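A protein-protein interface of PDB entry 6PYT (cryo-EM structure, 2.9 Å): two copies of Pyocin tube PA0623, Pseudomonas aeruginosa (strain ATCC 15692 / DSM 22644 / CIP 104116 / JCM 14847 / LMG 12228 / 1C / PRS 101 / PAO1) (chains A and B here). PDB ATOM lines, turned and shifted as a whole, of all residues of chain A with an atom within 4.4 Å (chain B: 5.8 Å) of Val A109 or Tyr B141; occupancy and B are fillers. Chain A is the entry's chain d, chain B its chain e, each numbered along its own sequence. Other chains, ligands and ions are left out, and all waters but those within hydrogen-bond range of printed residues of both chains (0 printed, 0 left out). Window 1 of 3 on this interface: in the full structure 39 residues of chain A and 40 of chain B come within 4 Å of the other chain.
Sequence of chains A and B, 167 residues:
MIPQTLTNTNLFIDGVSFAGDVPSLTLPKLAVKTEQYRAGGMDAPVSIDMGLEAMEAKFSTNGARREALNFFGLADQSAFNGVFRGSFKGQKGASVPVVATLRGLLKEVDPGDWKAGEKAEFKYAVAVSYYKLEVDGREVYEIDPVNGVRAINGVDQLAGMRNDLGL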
ATOM      1  N   LEU A  69     -25.199   5.247  22.504  1.00  0.00           N
ATOM      2  CA  LEU A  69     -24.710   5.044  23.862  1.00  0.00           C
ATOM      3  C   LEU A  69     -25.010   3.647  24.380  1.00  0.00           C
ATOM      4  O   LEU A  69     -24.264   3.130  25.213  1.00  0.00           O
ATOM      5  CB  LEU A  69     -25.318   6.074  24.810  1.00  0.00           C
ATOM      6  CG  LEU A  69     -24.847   7.518  24.728  1.00  0.00           C
ATOM      7  CD1 LEU A  69     -25.692   8.376  25.614  1.00  0.00           C
ATOM      8  CD2 LEU A  69     -23.417   7.605  25.163  1.00  0.00           C
ATOM      9  N   PHE A  72     -22.183   0.576  24.107  1.00  0.00           N
ATOM     10  CA  PHE A  72     -20.916   0.512  24.814  1.00  0.00           C
ATOM     11  C   PHE A  72     -20.870  -0.693  25.734  1.00  0.00           C
ATOM     12  O   PHE A  72     -21.811  -0.949  26.481  1.00  0.00           O
ATOM     13  CB  PHE A  72     -20.683   1.770  25.646  1.00  0.00           C
ATOM     14  CG  PHE A  72     -19.431   1.710  26.472  1.00  0.00           C
ATOM     15  CD1 PHE A  72     -18.202   1.882  25.879  1.00  0.00           C
ATOM     16  CD2 PHE A  72     -19.483   1.455  27.834  1.00  0.00           C
ATOM     17  CE1 PHE A  72     -17.053   1.806  26.621  1.00  0.00           C
ATOM     18  CE2 PHE A  72     -18.334   1.366  28.569  1.00  0.00           C
ATOM     19  CZ  PHE A  72     -17.122   1.551  27.963  1.00  0.00           C
ATOM     20  N   GLU A 108     -14.687   2.790  23.551  1.00  0.00           N
ATOM     21  CA  GLU A 108     -14.645   3.905  24.481  1.00  0.00           C
ATOM     22  C   GLU A 108     -15.681   4.948  24.107  1.00  0.00           C
ATOM     23  O   GLU A 108     -15.914   5.224  22.931  1.00  0.00           O
ATOM     24  CB  GLU A 108     -13.249   4.536  24.587  1.00  0.00           C
ATOM     25  N   VAL A 109     -16.333   5.478  25.131  1.00  0.00           N
ATOM     26  CA  VAL A 109     -17.230   6.615  25.024  1.00  0.00           C
ATOM     27  C   VAL A 109     -16.572   7.760  25.769  1.00  0.00           C
ATOM     28  O   VAL A 109     -16.283   7.644  26.963  1.00  0.00           O
ATOM     29  CB  VAL A 109     -18.614   6.301  25.600  1.00  0.00           C
ATOM     30  CG1 VAL A 109     -19.428   7.552  25.703  1.00  0.00           C
ATOM     31  CG2 VAL A 109     -19.319   5.300  24.725  1.00  0.00           C
ATOM     32  N   ASP A 110     -16.315   8.858  25.067  1.00  0.00           N
ATOM     33  CA  ASP A 110     -15.565   9.988  25.603  1.00  0.00           C
ATOM     34  C   ASP A 110     -16.445  11.229  25.546  1.00  0.00           C
ATOM     35  O   ASP A 110     -16.363  12.009  24.587  1.00  0.00           O
ATOM     36  CB  ASP A 110     -14.275  10.187  24.808  1.00  0.00           C
ATOM     37  N   PRO A 111     -17.302  11.445  26.544  1.00  0.00           N
ATOM     38  CA  PRO A 111     -17.920  12.768  26.691  1.00  0.00           C
ATOM     39  C   PRO A 111     -16.859  13.759  27.136  1.00  0.00           C
ATOM     40  O   PRO A 111     -16.232  13.590  28.183  1.00  0.00           O
ATOM     41  CB  PRO A 111     -18.990  12.545  27.761  1.00  0.00           C
ATOM     42  CG  PRO A 111     -18.539  11.376  28.506  1.00  0.00           C
ATOM     43  CD  PRO A 111     -17.804  10.503  27.556  1.00  0.00           C
ATOM     44  N   LYS A 123     -17.258  11.697  21.896  1.00  0.00           N
ATOM     45  CA  LYS A 123     -16.354  10.991  20.999  1.00  0.00           C
ATOM     46  C   LYS A 123     -16.410   9.501  21.291  1.00  0.00           C
ATOM     47  O   LYS A 123     -16.220   9.083  22.433  1.00  0.00           O
ATOM     48  CB  LYS A 123     -14.923  11.499  21.145  1.00  0.00           C
ATOM     49  CG  LYS A 123     -14.709  12.914  20.684  1.00  0.00           C
ATOM     50  CD  LYS A 123     -13.248  13.273  20.763  1.00  0.00           C
ATOM     51  CE  LYS A 123     -13.034  14.733  20.455  1.00  0.00           C
ATOM     52  NZ  LYS A 123     -13.380  15.069  19.054  1.00  0.00           N
ATOM     53  N   TYR A 124     -16.674   8.704  20.269  1.00  0.00           N
ATOM     54  CA  TYR A 124     -16.752   7.258  20.416  1.00  0.00           C
ATOM     55  C   TYR A 124     -15.602   6.626  19.646  1.00  0.00           C
ATOM     56  O   TYR A 124     -14.951   7.278  18.836  1.00  0.00           O
ATOM     57  CB  TYR A 124     -18.090   6.732  19.897  1.00  0.00           C
ATOM     58  CG  TYR A 124     -19.331   7.289  20.572  1.00  0.00           C
ATOM     59  CD1 TYR A 124     -19.322   7.798  21.857  1.00  0.00           C
ATOM     60  CD2 TYR A 124     -20.502   7.362  19.883  1.00  0.00           C
ATOM     61  CE1 TYR A 124     -20.483   8.322  22.419  1.00  0.00           C
ATOM     62  CE2 TYR A 124     -21.637   7.870  20.424  1.00  0.00           C
ATOM     63  CZ  TYR A 124     -21.637   8.351  21.687  1.00  0.00           C
ATOM     64  OH  TYR A 124     -22.796   8.859  22.207  1.00  0.00           O
ATOM     65  N   PRO B  28     -16.909  11.040  33.303  1.00  0.00           N
ATOM     66  CA  PRO B  28     -15.817  10.080  33.151  1.00  0.00           C
ATOM     67  C   PRO B  28     -15.827   9.401  31.795  1.00  0.00           C
ATOM     68  O   PRO B  28     -16.875   9.038  31.265  1.00  0.00           O
ATOM     69  CB  PRO B  28     -16.061   9.085  34.287  1.00  0.00           C
ATOM     70  CG  PRO B  28     -17.455   9.252  34.647  1.00  0.00           C
ATOM     71  CD  PRO B  28     -17.772  10.681  34.439  1.00  0.00           C
ATOM     72  N   LYS B  29     -14.639   9.275  31.218  1.00  0.00           N
ATOM     73  CA  LYS B  29     -14.467   8.582  29.950  1.00  0.00           C
ATOM     74  C   LYS B  29     -14.604   7.089  30.183  1.00  0.00           C
ATOM     75  O   LYS B  29     -13.750   6.470  30.822  1.00  0.00           O
ATOM     76  CB  LYS B  29     -13.109   8.919  29.346  1.00  0.00           C
ATOM     77  CG  LYS B  29     -12.831   8.239  28.033  1.00  0.00           C
ATOM     78  CD  LYS B  29     -11.576   8.796  27.393  1.00  0.00           C
ATOM     79  CE  LYS B  29     -10.320   8.308  28.072  1.00  0.00           C
ATOM     80  NZ  LYS B  29     -10.065   6.872  27.785  1.00  0.00           N
ATOM     81  N   LEU B  30     -15.686   6.512  29.689  1.00  0.00           N
ATOM     82  CA  LEU B  30     -15.890   5.077  29.794  1.00  0.00           C
ATOM     83  C   LEU B  30     -15.102   4.412  28.687  1.00  0.00           C
ATOM     84  O   LEU B  30     -15.502   4.467  27.527  1.00  0.00           O
ATOM     85  CB  LEU B  30     -17.360   4.706  29.672  1.00  0.00           C
ATOM     86  CG  LEU B  30     -18.307   4.897  30.838  1.00  0.00           C
ATOM     87  CD1 LEU B  30     -18.746   6.322  30.919  1.00  0.00           C
ATOM     88  CD2 LEU B  30     -19.482   4.020  30.622  1.00  0.00           C
ATOM     89  N   ALA B  31     -13.989   3.789  29.031  1.00  0.00           N
ATOM     90  CA  ALA B  31     -13.198   3.032  28.081  1.00  0.00           C
ATOM     91  C   ALA B  31     -13.152   1.596  28.559  1.00  0.00           C
ATOM     92  O   ALA B  31     -12.934   1.343  29.744  1.00  0.00           O
ATOM     93  CB  ALA B  31     -11.788   3.606  27.950  1.00  0.00           C
ATOM     94  N   TYR B 131     -20.984   5.125  39.059  1.00  0.00           N
ATOM     95  CA  TYR B 131     -21.355   6.028  37.983  1.00  0.00           C
ATOM     96  C   TYR B 131     -22.645   5.556  37.346  1.00  0.00           C
ATOM     97  O   TYR B 131     -22.714   4.428  36.863  1.00  0.00           O
ATOM     98  CB  TYR B 131     -20.240   6.112  36.951  1.00  0.00           C
ATOM     99  CG  TYR B 131     -20.576   6.983  35.781  1.00  0.00           C
ATOM    100  CD1 TYR B 131     -20.738   8.348  35.935  1.00  0.00           C
ATOM    101  CD2 TYR B 131     -20.692   6.450  34.516  1.00  0.00           C
ATOM    102  CE1 TYR B 131     -21.043   9.144  34.865  1.00  0.00           C
ATOM    103  CE2 TYR B 131     -20.998   7.238  33.450  1.00  0.00           C
ATOM    104  CZ  TYR B 131     -21.159   8.579  33.620  1.00  0.00           C
ATOM    105  OH  TYR B 131     -21.453   9.352  32.532  1.00  0.00           O
ATOM    106  N   LYS B 132     -23.659   6.415  37.348  1.00  0.00           N
ATOM    107  CA  LYS B 132     -24.906   6.144  36.650  1.00  0.00           C
ATOM    108  C   LYS B 132     -25.227   7.317  35.746  1.00  0.00           C
ATOM    109  O   LYS B 132     -25.377   8.441  36.221  1.00  0.00           O
ATOM    110  CB  LYS B 132     -26.062   5.900  37.618  1.00  0.00           C
ATOM    111  CG  LYS B 132     -27.338   5.545  36.893  1.00  0.00           C
ATOM    112  CD  LYS B 132     -28.446   5.115  37.812  1.00  0.00           C
ATOM    113  CE  LYS B 132     -29.084   6.292  38.490  1.00  0.00           C
ATOM    114  NZ  LYS B 132     -30.267   5.847  39.264  1.00  0.00           N
ATOM    115  N   LEU B 133     -25.347   7.052  34.456  1.00  0.00           N
ATOM    116  CA  LEU B 133     -25.717   8.059  33.474  1.00  0.00           C
ATOM    117  C   LEU B 133     -27.165   7.846  33.062  1.00  0.00           C
ATOM    118  O   LEU B 133     -27.513   6.779  32.554  1.00  0.00           O
ATOM    119  CB  LEU B 133     -24.803   7.975  32.258  1.00  0.00           C
ATOM    120  CG  LEU B 133     -25.035   8.996  31.158  1.00  0.00           C
ATOM    121  CD1 LEU B 133     -24.769  10.367  31.681  1.00  0.00           C
ATOM    122  CD2 LEU B 133     -24.139   8.697  29.996  1.00  0.00           C
ATOM    123  N   GLU B 134     -28.003   8.851  33.278  1.00  0.00           N
ATOM    124  CA  GLU B 134     -29.372   8.839  32.785  1.00  0.00           C
ATOM    125  C   GLU B 134     -29.519   9.873  31.684  1.00  0.00           C
ATOM    126  O   GLU B 134     -29.134  11.030  31.856  1.00  0.00           O
ATOM    127  CB  GLU B 134     -30.383   9.119  33.893  1.00  0.00           C
ATOM    128  N   GLU B 139     -32.050   5.122  32.298  1.00  0.00           N
ATOM    129  CA  GLU B 139     -30.721   4.644  32.667  1.00  0.00           C
ATOM    130  C   GLU B 139     -29.970   4.162  31.441  1.00  0.00           C
ATOM    131  O   GLU B 139     -30.395   3.214  30.775  1.00  0.00           O
ATOM    132  CB  GLU B 139     -30.815   3.510  33.680  1.00  0.00           C
ATOM    133  N   VAL B 140     -28.859   4.820  31.139  1.00  0.00           N
ATOM    134  CA  VAL B 140     -27.984   4.363  30.077  1.00  0.00           C
ATOM    135  C   VAL B 140     -26.880   3.542  30.716  1.00  0.00           C
ATOM    136  O   VAL B 140     -26.737   2.357  30.441  1.00  0.00           O
ATOM    137  CB  VAL B 140     -27.419   5.536  29.263  1.00  0.00           C
ATOM    138  CG1 VAL B 140     -26.503   5.028  28.190  1.00  0.00           C
ATOM    139  CG2 VAL B 140     -28.541   6.319  28.651  1.00  0.00           C
ATOM    140  N   TYR B 141     -26.106   4.141  31.598  1.00  0.00           N
ATOM    141  CA  TYR B 141     -24.974   3.448  32.186  1.00  0.00           C
ATOM    142  C   TYR B 141     -25.211   3.282  33.674  1.00  0.00           C
ATOM    143  O   TYR B 141     -25.900   4.085  34.294  1.00  0.00           O
ATOM    144  CB  TYR B 141     -23.689   4.219  31.927  1.00  0.00           C
ATOM    145  CG  TYR B 141     -23.309   4.257  30.477  1.00  0.00           C
ATOM    146  CD1 TYR B 141     -23.645   3.221  29.625  1.00  0.00           C
ATOM    147  CD2 TYR B 141     -22.702   5.373  29.940  1.00  0.00           C
ATOM    148  CE1 TYR B 141     -23.322   3.270  28.293  1.00  0.00           C
ATOM    149  CE2 TYR B 141     -22.382   5.432  28.610  1.00  0.00           C
ATOM    150  CZ  TYR B 141     -22.698   4.381  27.795  1.00  0.00           C
ATOM    151  OH  TYR B 141     -22.382   4.444  26.468  1.00  0.00           O
ATOM    152  N   GLU B 142     -24.666   2.210  34.232  1.00  0.00           N
ATOM    153  CA  GLU B 142     -24.616   2.050  35.681  1.00  0.00           C
ATOM    154  C   GLU B 142     -23.409   1.184  35.989  1.00  0.00           C
ATOM    155  O   GLU B 142     -23.437  -0.021  35.743  1.00  0.00           O
ATOM    156  CB  GLU B 142     -25.891   1.436  36.234  1.00  0.00           C
ATOM    157  N   ILE B 143     -22.353   1.796  36.507  1.00  0.00           N
ATOM    158  CA  ILE B 143     -21.080   1.123  36.717  1.00  0.00           C
ATOM    159  C   ILE B 143     -20.745   1.202  38.190  1.00  0.00           C
ATOM    160  O   ILE B 143     -20.553   2.293  38.734  1.00  0.00           O
ATOM    161  CB  ILE B 143     -19.943   1.720  35.876  1.00  0.00           C
ATOM    162  CG1 ILE B 143     -20.193   1.515  34.389  1.00  0.00           C
ATOM    163  CG2 ILE B 143     -18.645   1.056  36.235  1.00  0.00           C
ATOM    164  CD1 ILE B 143     -20.847   2.660  33.719  1.00  0.00           C
ATOM    165  N   ALA B 151     -24.360  -2.158  33.809  1.00  0.00           N
ATOM    166  CA  ALA B 151     -25.648  -2.130  33.134  1.00  0.00           C
ATOM    167  C   ALA B 151     -25.618  -1.133  31.984  1.00  0.00           C
ATOM    168  O   ALA B 151     -25.109  -0.022  32.132  1.00  0.00           O
ATOM    169  CB  ALA B 151     -26.757  -1.766  34.116  1.00  0.00           C
ATOM    170  N   ILE B 152     -26.158  -1.538  30.831  1.00  0.00           N
ATOM    171  CA  ILE B 152     -26.014  -0.760  29.603  1.00  0.00           C
ATOM    172  C   ILE B 152     -27.377  -0.324  29.063  1.00  0.00           C
ATOM    173  O   ILE B 152     -27.496   0.695  28.373  1.00  0.00           O
ATOM    174  CB  ILE B 152     -25.187  -1.553  28.569  1.00  0.00           C
ATOM    175  CG1 ILE B 152     -23.807  -1.862  29.137  1.00  0.00           C
ATOM    176  CG2 ILE B 152     -24.952  -0.784  27.290  1.00  0.00           C
ATOM    177  CD1 ILE B 152     -23.023  -0.652  29.542  1.00  0.00           C
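The side-chain hydroxyl (OH) of Tyr B141 sits at hydrogen-bond distance from the backbone carbonyl oxygen (O) of Leu A69. O of Leu B30 is in hydrogen-bond range of N of Val A109 (2.7 Å).
The backbone carbonyl oxygen of Tyr B141 lies within hydrogen-bond range of the backbone NH of Leu B133 (3.0 Å). O of Lys A123 sits at hydrogen-bond distance from N of Asp A110, at 2.6 Å. The backbone carbonyl oxygen (O) of Leu B133 sits at hydrogen-bond distance from the backbone NH (N) of Val B140 (2.8 Å).
Among the printed residues, pairs that only touch across the chains: Phe A72 with Leu B30, Glu A108 with Leu B30, Phe A72 with Ile B152, Phe A72 with Tyr B141, Val A109 with Lys B29, Val A109 with Tyr B141, Leu A69 with Val B140, Glu A108 with Ala B31, Pro A111 with Pro B28, Asp A110 with Lys B29 and Phe A72 with Ala B31.
Val A109 touches three residues of chain B. Of the printed residues of chain B, Asp A110 touches Lys B29. Lys A123 touches none of the printed residues of chain B. Printed residues of chain A within 4 Å of Leu B30: Phe A72, Glu A108 and Val A109. Printed residues of chain A within 4 Å of Ala B31: Phe A72 (3.996 Å) and Glu A108 (3.8 Å). Printed residues of chain A within 4 Å of Tyr B141: Leu A69 (2.6 Å), Phe A72 (3.3 Å) and Val A109 (3.6 Å). Ile B143 touches none of the printed residues of chain A. Printed residues of chain A within 4 Å of Ile B152: Phe A72 (3.2 Å). The nearest printed residue of chain A that does not touch Tyr B141 is Tyr A124 (5.9 Å). The nearest printed residue of chain B that does not touch Glu A108 is Lys B29 (5.1 Å).
Hydrophobic or aromatic side chains of chain B within 4 Å of the printed part of chain A: Leu B30, Ala B31, Val B140, Tyr B141 and Ile B152. Along chain A the printed residues that touch a printed residue of chain B span positions 69 to 111. Among the printed residues, no Asp or Glu carboxylate lies within 4 Å of a Lys or Arg side-chain nitrogen of the other chain.
No position is printed for both chains. Of the 13 pairs that touch across the chains among the printed residues, none has its exchanged pair printed and touching as well.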
